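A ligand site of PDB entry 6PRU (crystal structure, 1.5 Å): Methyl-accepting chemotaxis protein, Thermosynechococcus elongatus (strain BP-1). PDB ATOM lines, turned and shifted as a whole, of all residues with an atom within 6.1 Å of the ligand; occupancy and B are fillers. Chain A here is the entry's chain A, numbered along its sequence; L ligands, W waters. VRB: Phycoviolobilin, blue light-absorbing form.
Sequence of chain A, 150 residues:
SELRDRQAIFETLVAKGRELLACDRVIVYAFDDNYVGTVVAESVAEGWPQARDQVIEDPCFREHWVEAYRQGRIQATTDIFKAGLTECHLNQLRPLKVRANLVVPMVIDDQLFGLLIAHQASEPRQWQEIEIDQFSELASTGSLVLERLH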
ATOM      1  N   ILE A  27       8.024 -20.292  -1.062  1.00  0.00           N
ATOM      2  CA  ILE A  27       6.882 -19.528  -1.543  1.00  0.00           C
ATOM      3  C   ILE A  27       5.818 -20.449  -2.112  1.00  0.00           C
ATOM      4  O   ILE A  27       6.068 -21.591  -2.551  1.00  0.00           O
ATOM      5  CB  ILE A  27       7.314 -18.483  -2.626  1.00  0.00           C
ATOM      6  CG1 ILE A  27       7.990 -19.208  -3.804  1.00  0.00           C
ATOM      7  CG2 ILE A  27       8.231 -17.489  -2.081  1.00  0.00           C
ATOM      8  CD1 ILE A  27       8.205 -18.290  -5.035  1.00  0.00           C
ATOM      9  N   TYR A  29       3.621 -20.158  -5.419  1.00  0.00           N
ATOM     10  CA  TYR A  29       3.550 -19.443  -6.716  1.00  0.00           C
ATOM     11  C   TYR A  29       2.307 -19.916  -7.457  1.00  0.00           C
ATOM     12  O   TYR A  29       2.247 -21.040  -7.948  1.00  0.00           O
ATOM     13  CB  TYR A  29       4.874 -19.746  -7.429  1.00  0.00           C
ATOM     14  CG  TYR A  29       5.108 -19.165  -8.800  1.00  0.00           C
ATOM     15  CD1 TYR A  29       5.467 -17.831  -8.978  1.00  0.00           C
ATOM     16  CD2 TYR A  29       5.002 -19.945  -9.874  1.00  0.00           C
ATOM     17  CE1 TYR A  29       5.682 -17.259 -10.242  1.00  0.00           C
ATOM     18  CE2 TYR A  29       5.216 -19.399 -11.156  1.00  0.00           C
ATOM     19  CZ  TYR A  29       5.575 -18.097 -11.311  1.00  0.00           C
ATOM     20  OH  TYR A  29       5.807 -17.600 -12.608  1.00  0.00           O
ATOM     21  N   VAL A  39       3.392 -14.609  -6.454  1.00  0.00           N
ATOM     22  CA  VAL A  39       3.879 -15.133  -5.136  1.00  0.00           C
ATOM     23  C   VAL A  39       2.821 -14.744  -4.110  1.00  0.00           C
ATOM     24  O   VAL A  39       2.701 -13.584  -3.726  1.00  0.00           O
ATOM     25  CB  VAL A  39       5.232 -14.549  -4.801  1.00  0.00           C
ATOM     26  CG1 VAL A  39       5.739 -15.111  -3.432  1.00  0.00           C
ATOM     27  CG2 VAL A  39       6.223 -14.803  -5.899  1.00  0.00           C
ATOM     28  N   ILE A  56       5.298 -12.717 -11.628  1.00  0.00           N
ATOM     29  CA  ILE A  56       6.417 -13.129 -12.429  1.00  0.00           C
ATOM     30  C   ILE A  56       5.830 -13.920 -13.603  1.00  0.00           C
ATOM     31  O   ILE A  56       5.249 -14.986 -13.403  1.00  0.00           O
ATOM     32  CB  ILE A  56       7.429 -13.988 -11.640  1.00  0.00           C
ATOM     33  CG1 ILE A  56       7.947 -13.172 -10.469  1.00  0.00           C
ATOM     34  CG2 ILE A  56       8.536 -14.441 -12.583  1.00  0.00           C
ATOM     35  CD1 ILE A  56       8.832 -13.969  -9.547  1.00  0.00           C
ATOM     36  N   GLU A  57       5.984 -13.391 -14.809  1.00  0.00           N
ATOM     37  CA  GLU A  57       5.520 -14.096 -16.013  1.00  0.00           C
ATOM     38  C   GLU A  57       6.671 -14.834 -16.615  1.00  0.00           C
ATOM     39  O   GLU A  57       7.615 -14.233 -17.170  1.00  0.00           O
ATOM     40  CB  GLU A  57       4.910 -13.119 -17.001  1.00  0.00           C
ATOM     41  CG  GLU A  57       4.683 -13.824 -18.385  1.00  0.00           C
ATOM     42  CD  GLU A  57       3.766 -13.079 -19.293  1.00  0.00           C
ATOM     43  OE1 GLU A  57       3.656 -11.839 -19.140  1.00  0.00           O
ATOM     44  OE2 GLU A  57       3.167 -13.714 -20.185  1.00  0.00           O
ATOM     45  N   ASP A  58       6.590 -16.177 -16.576  1.00  0.00           N
ATOM     46  CA  ASP A  58       7.589 -17.007 -17.192  1.00  0.00           C
ATOM     47  C   ASP A  58       6.899 -17.967 -18.141  1.00  0.00           C
ATOM     48  O   ASP A  58       6.087 -18.810 -17.711  1.00  0.00           O
ATOM     49  CB  ASP A  58       8.349 -17.715 -16.084  1.00  0.00           C
ATOM     50  CG  ASP A  58       9.457 -18.609 -16.596  1.00  0.00           C
ATOM     51  OD1 ASP A  58       9.475 -18.911 -17.774  1.00  0.00           O
ATOM     52  OD2 ASP A  58      10.284 -19.005 -15.704  1.00  0.00           O
ATOM     53  N   PRO A  59       7.082 -17.774 -19.450  1.00  0.00           N
ATOM     54  CA  PRO A  59       6.317 -18.555 -20.428  1.00  0.00           C
ATOM     55  C   PRO A  59       6.711 -20.027 -20.484  1.00  0.00           C
ATOM     56  O   PRO A  59       6.020 -20.819 -21.135  1.00  0.00           O
ATOM     57  CB  PRO A  59       6.616 -17.841 -21.749  1.00  0.00           C
ATOM     58  CG  PRO A  59       7.898 -17.189 -21.560  1.00  0.00           C
ATOM     59  CD  PRO A  59       8.034 -16.854 -20.077  1.00  0.00           C
ATOM     60  N   CYS A  60       7.766 -20.458 -19.784  1.00  0.00           N
ATOM     61  CA  CYS A  60       8.171 -21.834 -20.046  1.00  0.00           C
ATOM     62  C   CYS A  60       7.116 -22.799 -19.520  1.00  0.00           C
ATOM     63  O   CYS A  60       6.976 -23.903 -20.073  1.00  0.00           O
ATOM     64  CB  CYS A  60       9.537 -22.162 -19.469  1.00  0.00           C
ATOM     65  SG  CYS A  60       9.521 -22.328 -17.641  1.00  0.00           S
ATOM     66  N   PHE A  61       6.397 -22.450 -18.452  1.00  0.00           N
ATOM     67  CA  PHE A  61       5.384 -23.344 -17.929  1.00  0.00           C
ATOM     68  C   PHE A  61       4.285 -23.624 -18.926  1.00  0.00           C
ATOM     69  O   PHE A  61       4.035 -24.790 -19.294  1.00  0.00           O
ATOM     70  CB  PHE A  61       4.844 -22.812 -16.603  1.00  0.00           C
ATOM     71  CG  PHE A  61       5.889 -22.706 -15.540  1.00  0.00           C
ATOM     72  CD1 PHE A  61       6.431 -23.821 -14.981  1.00  0.00           C
ATOM     73  CD2 PHE A  61       6.372 -21.468 -15.133  1.00  0.00           C
ATOM     74  CE1 PHE A  61       7.425 -23.699 -14.051  1.00  0.00           C
ATOM     75  CE2 PHE A  61       7.345 -21.359 -14.204  1.00  0.00           C
ATOM     76  CZ  PHE A  61       7.876 -22.486 -13.662  1.00  0.00           C
ATOM     77  N   GLU A  63       4.258 -23.104 -22.087  1.00  0.00           N
ATOM     78  CA  GLU A  63       4.711 -23.552 -23.384  1.00  0.00           C
ATOM     79  C   GLU A  63       5.248 -24.978 -23.354  1.00  0.00           C
ATOM     80  O   GLU A  63       5.297 -25.615 -24.414  1.00  0.00           O
ATOM     81  CB  GLU A  63       5.786 -22.599 -23.927  1.00  0.00           C
ATOM     82  CG  GLU A  63       5.185 -21.223 -24.215  1.00  0.00           C
ATOM     83  CD  GLU A  63       6.159 -20.260 -24.848  1.00  0.00           C
ATOM     84  OE1 GLU A  63       7.358 -20.584 -24.949  1.00  0.00           O
ATOM     85  OE2 GLU A  63       5.698 -19.171 -25.254  1.00  0.00           O
ATOM     86  N   HIS A  64       5.655 -25.461 -22.187  1.00  0.00           N
ATOM     87  CA  HIS A  64       6.265 -26.806 -22.144  1.00  0.00           C
ATOM     88  C   HIS A  64       5.827 -27.729 -21.013  1.00  0.00           C
ATOM     89  O   HIS A  64       5.847 -28.973 -21.209  1.00  0.00           O
ATOM     90  CB  HIS A  64       7.772 -26.638 -22.019  1.00  0.00           C
ATOM     91  CG  HIS A  64       8.393 -25.902 -23.180  1.00  0.00           C
ATOM     92  ND1 HIS A  64       9.267 -24.843 -23.040  1.00  0.00           N
ATOM     93  CD2 HIS A  64       8.272 -26.136 -24.491  1.00  0.00           C
ATOM     94  CE1 HIS A  64       9.638 -24.435 -24.251  1.00  0.00           C
ATOM     95  NE2 HIS A  64       9.035 -25.192 -25.141  1.00  0.00           N
ATOM     96  N   TRP A  65       5.476 -27.196 -19.868  1.00  0.00           N
ATOM     97  CA  TRP A  65       5.573 -28.017 -18.630  1.00  0.00           C
ATOM     98  C   TRP A  65       4.326 -28.164 -17.802  1.00  0.00           C
ATOM     99  O   TRP A  65       4.355 -28.855 -16.830  1.00  0.00           O
ATOM    100  CB  TRP A  65       6.699 -27.497 -17.710  1.00  0.00           C
ATOM    101  CG  TRP A  65       8.025 -27.436 -18.366  1.00  0.00           C
ATOM    102  CD1 TRP A  65       8.817 -26.344 -18.556  1.00  0.00           C
ATOM    103  CD2 TRP A  65       8.705 -28.531 -19.015  1.00  0.00           C
ATOM    104  NE1 TRP A  65       9.910 -26.663 -19.300  1.00  0.00           N
ATOM    105  CE2 TRP A  65       9.886 -27.999 -19.589  1.00  0.00           C
ATOM    106  CE3 TRP A  65       8.411 -29.872 -19.218  1.00  0.00           C
ATOM    107  CZ2 TRP A  65      10.785 -28.799 -20.286  1.00  0.00           C
ATOM    108  CZ3 TRP A  65       9.301 -30.639 -19.938  1.00  0.00           C
ATOM    109  CH2 TRP A  65      10.472 -30.100 -20.468  1.00  0.00           C
ATOM    110  N   TYR A  69       3.969 -31.006 -14.870  1.00  0.00           N
ATOM    111  CA  TYR A  69       3.862 -30.741 -13.438  1.00  0.00           C
ATOM    112  C   TYR A  69       2.558 -31.339 -12.874  1.00  0.00           C
ATOM    113  O   TYR A  69       2.555 -31.823 -11.755  1.00  0.00           O
ATOM    114  CB  TYR A  69       3.961 -29.227 -13.157  1.00  0.00           C
ATOM    115  CG  TYR A  69       5.358 -28.756 -13.026  1.00  0.00           C
ATOM    116  CD1 TYR A  69       6.093 -28.992 -11.865  1.00  0.00           C
ATOM    117  CD2 TYR A  69       6.018 -28.102 -14.043  1.00  0.00           C
ATOM    118  CE1 TYR A  69       7.368 -28.573 -11.741  1.00  0.00           C
ATOM    119  CE2 TYR A  69       7.313 -27.692 -13.914  1.00  0.00           C
ATOM    120  CZ  TYR A  69       8.007 -27.964 -12.737  1.00  0.00           C
ATOM    121  OH  TYR A  69       9.281 -27.575 -12.604  1.00  0.00           O
ATOM    122  N   ARG A  73       6.009 -33.907 -12.109  1.00  0.00           N
ATOM    123  CA  ARG A  73       7.325 -33.332 -12.348  1.00  0.00           C
ATOM    124  C   ARG A  73       7.715 -32.413 -11.210  1.00  0.00           C
ATOM    125  O   ARG A  73       6.882 -31.734 -10.626  1.00  0.00           O
ATOM    126  CB  ARG A  73       7.296 -32.544 -13.663  1.00  0.00           C
ATOM    127  CG  ARG A  73       8.689 -32.006 -14.087  1.00  0.00           C
ATOM    128  CD  ARG A  73       8.463 -31.138 -15.280  1.00  0.00           C
ATOM    129  NE  ARG A  73       9.745 -30.592 -15.831  1.00  0.00           N
ATOM    130  CZ  ARG A  73      10.487 -31.208 -16.705  1.00  0.00           C
ATOM    131  NH1 ARG A  73      10.243 -32.496 -17.072  1.00  0.00           N
ATOM    132  NH2 ARG A  73      11.572 -30.577 -17.213  1.00  0.00           N
ATOM    133  N   ILE A  74       9.010 -32.365 -10.967  1.00  0.00           N
ATOM    134  CA  ILE A  74       9.648 -31.421 -10.091  1.00  0.00           C
ATOM    135  C   ILE A  74      10.773 -30.728 -10.854  1.00  0.00           C
ATOM    136  O   ILE A  74      11.071 -31.062 -11.982  1.00  0.00           O
ATOM    137  CB  ILE A  74      10.221 -32.091  -8.818  1.00  0.00           C
ATOM    138  CG1 ILE A  74      11.435 -32.847  -9.137  1.00  0.00           C
ATOM    139  CG2 ILE A  74       9.065 -32.840  -8.100  1.00  0.00           C
ATOM    140  CD1 ILE A  74      12.121 -33.420  -7.864  1.00  0.00           C
ATOM    141  N   GLN A  75      11.331 -29.708 -10.217  1.00  0.00           N
ATOM    142  CA  GLN A  75      12.654 -29.187 -10.614  1.00  0.00           C
ATOM    143  C   GLN A  75      13.537 -29.174  -9.379  1.00  0.00           C
ATOM    144  O   GLN A  75      13.207 -28.526  -8.380  1.00  0.00           O
ATOM    145  CB  GLN A  75      12.583 -27.730 -11.164  1.00  0.00           C
ATOM    146  CG  GLN A  75      13.980 -27.130 -11.400  1.00  0.00           C
ATOM    147  CD  GLN A  75      14.604 -27.557 -12.680  1.00  0.00           C
ATOM    148  OE1 GLN A  75      14.111 -27.257 -13.761  1.00  0.00           O
ATOM    149  NE2 GLN A  75      15.689 -28.397 -12.575  1.00  0.00           N
ATOM    150  N   LEU A  85      20.955 -21.918 -18.104  1.00  0.00           N
ATOM    151  CA  LEU A  85      19.821 -21.013 -18.205  1.00  0.00           C
ATOM    152  C   LEU A  85      20.151 -19.773 -19.007  1.00  0.00           C
ATOM    153  O   LEU A  85      21.295 -19.317 -19.091  1.00  0.00           O
ATOM    154  CB  LEU A  85      19.358 -20.626 -16.789  1.00  0.00           C
ATOM    155  CG  LEU A  85      18.980 -21.820 -15.909  1.00  0.00           C
ATOM    156  CD1 LEU A  85      18.778 -21.369 -14.498  1.00  0.00           C
ATOM    157  CD2 LEU A  85      17.742 -22.517 -16.412  1.00  0.00           C
ATOM    158  N   THR A  86      19.112 -19.206 -19.620  1.00  0.00           N
ATOM    159  CA  THR A  86      19.272 -17.979 -20.394  1.00  0.00           C
ATOM    160  C   THR A  86      19.289 -16.780 -19.461  1.00  0.00           C
ATOM    161  O   THR A  86      18.918 -16.873 -18.292  1.00  0.00           O
ATOM    162  CB  THR A  86      18.135 -17.833 -21.403  1.00  0.00           C
ATOM    163  OG1 THR A  86      16.897 -17.680 -20.706  1.00  0.00           O
ATOM    164  CG2 THR A  86      18.077 -19.109 -22.291  1.00  0.00           C
ATOM    165  N   GLU A  87      19.759 -15.646 -19.979  1.00  0.00           N
ATOM    166  CA  GLU A  87      19.754 -14.425 -19.185  1.00  0.00           C
ATOM    167  C   GLU A  87      18.340 -14.035 -18.779  1.00  0.00           C
ATOM    168  O   GLU A  87      18.127 -13.513 -17.679  1.00  0.00           O
ATOM    169  CB  GLU A  87      20.442 -13.289 -19.947  1.00  0.00           C
ATOM    170  CG  GLU A  87      20.161 -11.893 -19.382  1.00  0.00           C
ATOM    171  CD  GLU A  87      20.502 -11.723 -17.897  1.00  0.00           C
ATOM    172  OE1 GLU A  87      19.987 -10.765 -17.278  1.00  0.00           O
ATOM    173  OE2 GLU A  87      21.253 -12.536 -17.342  1.00  0.00           O
ATOM    174  N   CYS A  88      17.353 -14.271 -19.663  1.00  0.00           N
ATOM    175  CA  CYS A  88      15.976 -13.962 -19.299  1.00  0.00           C
ATOM    176  C   CYS A  88      15.587 -14.683 -18.007  1.00  0.00           C
ATOM    177  O   CYS A  88      15.024 -14.080 -17.079  1.00  0.00           O
ATOM    178  CB  CYS A  88      15.011 -14.346 -20.435  1.00  0.00           C
ATOM    179  SG  CYS A  88      13.322 -13.739 -20.166  1.00  0.00           S
ATOM    180  N   HIS A  89      15.898 -15.958 -17.931  1.00  0.00           N
ATOM    181  CA  HIS A  89      15.607 -16.727 -16.719  1.00  0.00           C
ATOM    182  C   HIS A  89      16.425 -16.209 -15.540  1.00  0.00           C
ATOM    183  O   HIS A  89      15.884 -15.959 -14.466  1.00  0.00           O
ATOM    184  CB  HIS A  89      15.919 -18.212 -16.948  1.00  0.00           C
ATOM    185  CG  HIS A  89      15.422 -19.118 -15.864  1.00  0.00           C
ATOM    186  ND1 HIS A  89      14.489 -20.099 -16.085  1.00  0.00           N
ATOM    187  CD2 HIS A  89      15.763 -19.208 -14.548  1.00  0.00           C
ATOM    188  CE1 HIS A  89      14.240 -20.744 -14.940  1.00  0.00           C
ATOM    189  NE2 HIS A  89      14.987 -20.216 -13.987  1.00  0.00           N
ATOM    190  N   GLN A  92      15.109 -12.987 -14.079  1.00  0.00           N
ATOM    191  CA  GLN A  92      13.888 -12.956 -13.295  1.00  0.00           C
ATOM    192  C   GLN A  92      14.140 -13.374 -11.873  1.00  0.00           C
ATOM    193  O   GLN A  92      13.369 -13.039 -10.978  1.00  0.00           O
ATOM    194  CB  GLN A  92      12.784 -13.786 -13.978  1.00  0.00           C
ATOM    195  CG  GLN A  92      12.802 -15.229 -13.733  1.00  0.00           C
ATOM    196  CD  GLN A  92      11.888 -16.016 -14.690  1.00  0.00           C
ATOM    197  OE1 GLN A  92      10.967 -15.465 -15.357  1.00  0.00           O
ATOM    198  NE2 GLN A  92      12.157 -17.319 -14.789  1.00  0.00           N
ATOM    199  N   LEU A  93      15.207 -14.197 -11.644  1.00  0.00           N
ATOM    200  CA  LEU A  93      15.567 -14.653 -10.322  1.00  0.00           C
ATOM    201  C   LEU A  93      16.504 -13.704  -9.583  1.00  0.00           C
ATOM    202  O   LEU A  93      16.508 -13.684  -8.348  1.00  0.00           O
ATOM    203  CB  LEU A  93      16.265 -16.015 -10.368  1.00  0.00           C
ATOM    204  CG  LEU A  93      15.483 -17.132 -11.027  1.00  0.00           C
ATOM    205  CD1 LEU A  93      16.284 -18.423 -10.956  1.00  0.00           C
ATOM    206  CD2 LEU A  93      14.112 -17.322 -10.448  1.00  0.00           C
ATOM    207  N   LEU A  96      15.466 -11.720  -6.551  1.00  0.00           N
ATOM    208  CA  LEU A  96      15.074 -12.511  -5.407  1.00  0.00           C
ATOM    209  C   LEU A  96      16.264 -13.092  -4.689  1.00  0.00           C
ATOM    210  O   LEU A  96      16.244 -13.187  -3.444  1.00  0.00           O
ATOM    211  CB  LEU A  96      14.153 -13.658  -5.890  1.00  0.00           C
ATOM    212  CG  LEU A  96      12.730 -13.291  -6.247  1.00  0.00           C
ATOM    213  CD1 LEU A  96      12.618 -12.582  -7.588  1.00  0.00           C
ATOM    214  CD2 LEU A  96      11.841 -14.536  -6.252  1.00  0.00           C
ATOM    215  N   VAL A  98      18.522 -16.340  -5.951  1.00  0.00           N
ATOM    216  CA  VAL A  98      18.325 -17.822  -6.004  1.00  0.00           C
ATOM    217  C   VAL A  98      19.622 -18.420  -6.478  1.00  0.00           C
ATOM    218  O   VAL A  98      20.070 -18.136  -7.602  1.00  0.00           O
ATOM    219  CB  VAL A  98      17.184 -18.171  -6.962  1.00  0.00           C
ATOM    220  CG1 VAL A  98      16.947 -19.697  -6.958  1.00  0.00           C
ATOM    221  CG2 VAL A  98      15.909 -17.473  -6.587  1.00  0.00           C
ATOM    222  N   ASN A 101      17.302 -24.289  -6.252  1.00  0.00           N
ATOM    223  CA  ASN A 101      15.904 -24.270  -6.034  1.00  0.00           C
ATOM    224  C   ASN A 101      15.260 -25.633  -6.210  1.00  0.00           C
ATOM    225  O   ASN A 101      15.797 -26.517  -6.846  1.00  0.00           O
ATOM    226  CB  ASN A 101      15.117 -23.249  -6.900  1.00  0.00           C
ATOM    227  CG  ASN A 101      15.399 -23.343  -8.362  1.00  0.00           C
ATOM    228  OD1 ASN A 101      16.180 -24.139  -8.835  1.00  0.00           O
ATOM    229  ND2 ASN A 101      14.635 -22.544  -9.141  1.00  0.00           N
ATOM    230  N   VAL A 103      11.265 -27.147  -6.820  1.00  0.00           N
ATOM    231  CA  VAL A 103       9.951 -26.763  -7.304  1.00  0.00           C
ATOM    232  C   VAL A 103       9.082 -28.015  -7.317  1.00  0.00           C
ATOM    233  O   VAL A 103       9.435 -28.987  -7.995  1.00  0.00           O
ATOM    234  CB  VAL A 103      10.055 -26.180  -8.709  1.00  0.00           C
ATOM    235  CG1 VAL A 103       8.700 -25.785  -9.297  1.00  0.00           C
ATOM    236  CG2 VAL A 103      11.023 -24.963  -8.722  1.00  0.00           C
ATOM    237  N   LEU A 115       2.804 -23.815  -7.766  1.00  0.00           N
ATOM    238  CA  LEU A 115       4.026 -24.525  -7.377  1.00  0.00           C
ATOM    239  C   LEU A 115       4.385 -24.084  -5.978  1.00  0.00           C
ATOM    240  O   LEU A 115       4.285 -22.910  -5.591  1.00  0.00           O
ATOM    241  CB  LEU A 115       5.210 -24.104  -8.340  1.00  0.00           C
ATOM    242  CG  LEU A 115       4.848 -24.301  -9.830  1.00  0.00           C
ATOM    243  CD1 LEU A 115       5.889 -23.676 -10.739  1.00  0.00           C
ATOM    244  CD2 LEU A 115       4.697 -25.853 -10.181  1.00  0.00           C
ATOM    245  N   ILE A 117       7.740 -23.699  -3.881  1.00  0.00           N
ATOM    246  CA  ILE A 117       9.102 -23.501  -4.329  1.00  0.00           C
ATOM    247  C   ILE A 117       9.995 -23.163  -3.157  1.00  0.00           C
ATOM    248  O   ILE A 117       9.702 -22.229  -2.393  1.00  0.00           O
ATOM    249  CB  ILE A 117       9.205 -22.413  -5.397  1.00  0.00           C
ATOM    250  CG1 ILE A 117       8.330 -22.805  -6.592  1.00  0.00           C
ATOM    251  CG2 ILE A 117      10.657 -22.218  -5.796  1.00  0.00           C
ATOM    252  CD1 ILE A 117       8.360 -21.770  -7.753  1.00  0.00           C
ATOM    253  N   ALA A 118      11.125 -23.871  -3.039  1.00  0.00           N
ATOM    254  CA  ALA A 118      12.135 -23.572  -2.052  1.00  0.00           C
ATOM    255  C   ALA A 118      13.378 -22.965  -2.708  1.00  0.00           C
ATOM    256  O   ALA A 118      13.793 -23.427  -3.771  1.00  0.00           O
ATOM    257  CB  ALA A 118      12.583 -24.861  -1.327  1.00  0.00           C
ATOM    258  N   HIS A 119      13.965 -21.963  -2.095  1.00  0.00           N
ATOM    259  CA  HIS A 119      15.230 -21.356  -2.529  1.00  0.00           C
ATOM    260  C   HIS A 119      16.298 -21.476  -1.437  1.00  0.00           C
ATOM    261  O   HIS A 119      16.050 -21.181  -0.258  1.00  0.00           O
ATOM    262  CB  HIS A 119      15.044 -19.835  -2.825  1.00  0.00           C
ATOM    263  CG  HIS A 119      14.120 -19.576  -3.960  1.00  0.00           C
ATOM    264  ND1 HIS A 119      13.405 -18.392  -4.056  1.00  0.00           N
ATOM    265  CD2 HIS A 119      13.796 -20.313  -5.034  1.00  0.00           C
ATOM    266  CE1 HIS A 119      12.713 -18.392  -5.183  1.00  0.00           C
ATOM    267  NE2 HIS A 119      12.891 -19.564  -5.784  1.00  0.00           N
HETATM  268  C01 VRB L   1      11.237 -14.685 -18.729  1.00  0.00           C
HETATM  269  C02 VRB L   1      12.496 -15.150 -19.446  1.00  0.00           C
HETATM  270  C03 VRB L   1      12.152 -16.249 -20.405  1.00  0.00           C
HETATM  271  C04 VRB L   1      11.333 -16.150 -21.451  1.00  0.00           C
HETATM  272  C05 VRB L   1      10.555 -14.961 -21.932  1.00  0.00           C
HETATM  273  C06 VRB L   1      11.286 -17.500 -22.014  1.00  0.00           C
HETATM  274  O07 VRB L   1      10.617 -17.775 -22.992  1.00  0.00           O
HETATM  275  N08 VRB L   1      12.035 -18.403 -21.345  1.00  0.00           N
HETATM  276  C09 VRB L   1      12.719 -17.677 -20.275  1.00  0.00           C
HETATM  277  C10 VRB L   1      12.557 -18.210 -18.905  1.00  0.00           C
HETATM  278  C11 VRB L   1      12.702 -19.713 -18.756  1.00  0.00           C
HETATM  279  C12 VRB L   1      13.671 -20.584 -19.157  1.00  0.00           C
HETATM  280  C13 VRB L   1      14.915 -20.233 -19.960  1.00  0.00           C
HETATM  281  C14 VRB L   1      13.326 -21.878 -18.736  1.00  0.00           C
HETATM  282  C15 VRB L   1      12.126 -21.747 -18.050  1.00  0.00           C
HETATM  283  C16 VRB L   1      11.250 -22.831 -17.307  1.00  0.00           C
HETATM  284  C17 VRB L   1      11.292 -22.601 -15.818  1.00  0.00           C
HETATM  285  C18 VRB L   1      11.581 -23.618 -14.877  1.00  0.00           C
HETATM  286  C19 VRB L   1      11.944 -25.027 -15.237  1.00  0.00           C
HETATM  287  C20 VRB L   1      10.754 -25.871 -15.500  1.00  0.00           C
HETATM  288  C21 VRB L   1      11.177 -27.352 -15.686  1.00  0.00           C
HETATM  289  O22 VRB L   1      10.602 -28.105 -14.835  1.00  0.00           O
HETATM  290  O23 VRB L   1      11.844 -27.798 -16.583  1.00  0.00           O
HETATM  291  C24 VRB L   1      11.501 -23.055 -13.614  1.00  0.00           C
HETATM  292  C25 VRB L   1      11.142 -21.661 -13.800  1.00  0.00           C
HETATM  293  N26 VRB L   1      11.075 -21.458 -15.121  1.00  0.00           N
HETATM  294  C27 VRB L   1      10.837 -20.507 -12.922  1.00  0.00           C
HETATM  295  C28 VRB L   1      11.038 -20.280 -11.585  1.00  0.00           C
HETATM  296  N29 VRB L   1      11.971 -20.826 -10.674  1.00  0.00           N
HETATM  297  C30 VRB L   1      11.799 -20.298  -9.494  1.00  0.00           C
HETATM  298  O31 VRB L   1      12.473 -20.539  -8.462  1.00  0.00           O
HETATM  299  C32 VRB L   1      10.737 -19.351  -9.554  1.00  0.00           C
HETATM  300  C33 VRB L   1      10.294 -19.339 -10.860  1.00  0.00           C
HETATM  301  C34 VRB L   1       9.154 -18.493 -11.400  1.00  0.00           C
HETATM  302  C35 VRB L   1      10.174 -18.519  -8.446  1.00  0.00           C
HETATM  303  C36 VRB L   1      10.985 -17.274  -8.290  1.00  0.00           C
HETATM  304  C37 VRB L   1      11.702 -23.815 -12.289  1.00  0.00           C
HETATM  305  N38 VRB L   1      11.736 -20.436 -18.063  1.00  0.00           N
HETATM  306  C39 VRB L   1      14.155 -23.135 -18.974  1.00  0.00           C
HETATM  307  C40 VRB L   1      13.960 -23.776 -20.370  1.00  0.00           C
HETATM  308  C41 VRB L   1      12.545 -24.129 -20.697  1.00  0.00           C
HETATM  309  O42 VRB L   1      11.990 -23.650 -21.671  1.00  0.00           O
HETATM  310  O43 VRB L   1      11.869 -24.936 -19.890  1.00  0.00           O
HETATM  311  O   HOH W   1      11.745 -20.986 -22.302  1.00  0.00           O
HETATM  312  O   HOH W   2      15.046 -17.375 -22.538  1.00  0.00           O
HETATM  313  O   HOH W   3      13.371 -26.694 -18.364  1.00  0.00           O
HETATM  314  O   HOH W   4       9.218 -20.849 -23.333  1.00  0.00           O
HETATM  315  O   HOH W   5      13.795 -19.981 -23.558  1.00  0.00           O
HETATM  316  O   HOH W   6      14.014 -24.087 -23.956  1.00  0.00           O
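An oxygen (O22) of the ligand lies within salt-bridge range of the guanidinium group of Arg 73, at 2.8 Å. A ring nitrogen (NE2) of His 119 sits at hydrogen-bond distance from an oxygen (O31) of the ligand (2.9 Å). ND2 of Asn 101 lies within hydrogen-bond range of O31 of the ligand (3.0 Å). OD2 of Asp 58 lies within hydrogen-bond range of N26 of the ligand, at 2.6 Å. The side-chain sulfur (SG) of Cys 60 is bonded to a carbon (C16) of the ligand. A nitrogen (N38) of the ligand sits close to a ring nitrogen (ND1) of His 89, 3.4 Å away. O43 of the ligand lies within hydrogen-bond range of NE1 of Trp 65 (2.7 Å). The side-chain sulfur of Cys 88 is covalently linked to a carbon (C02) of the ligand (1.8 Å). An oxygen (O42) of the ligand lies within hydrogen-bond range of a ring nitrogen (ND1) of His 64. An oxygen (O22) of the ligand lies within hydrogen-bond range of the side-chain hydroxyl (OH) of Tyr 69 (2.6 Å).
NE2 of Gln 92 lies within hydrogen-bond range of OD2 of Asp 58 (2.7 Å). N of Tyr 29 is in hydrogen-bond range of O of Leu 115 (2.8 Å). The backbone NH (N) of Cys 60 is in hydrogen-bond range of the side-chain carboxylate (OD1) of Asp 58 (3.1 Å). The backbone NH (N) of His 89 is in hydrogen-bond range of the side-chain hydroxyl (OG1) of Thr 86, at 3.4 Å. O of Ile 117 sits at hydrogen-bond distance from N of Ile 27 (2.9 Å). The backbone carbonyl oxygen of Gln 75 lies within hydrogen-bond range of the backbone NH of Val 103, 2.8 Å away. The side-chain hydroxyl of Tyr 29 lies within hydrogen-bond range of the backbone carbonyl oxygen of Ile 56 (2.8 Å).
Residues that only touch the ligand: Pro 59 (3.1 Å), Thr 86 (3.3 Å), Phe 61 (3.4 Å), Gln 75 (3.4 Å), Gln 92 (3.5 Å), Leu 96 (3.5 Å), Tyr 29 (3.6 Å), Ile 117 (3.6 Å), Leu 93 (3.8 Å), Val 103 (3.8 Å), Ile 27 (3.9 Å) and Glu 57 (3.97 Å). Hydrophobic or aromatic side chains that line the ligand: Ile 27, Tyr 29, Pro 59, Phe 61, His 64, Trp 65, Tyr 69, His 89, Leu 93, Leu 96, Val 103, Ile 117 and His 119. Of the 31 residues printed, 22 come within 4 Å of the ligand.
Water W2 lies within hydrogen-bond range of OG1 of Thr 86 and N08 of the ligand. Water W4 bridges the side-chain carboxylate (OE1) of Glu 63 (2.5 Å) and an oxygen (O07) of the ligand (3.4 Å).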
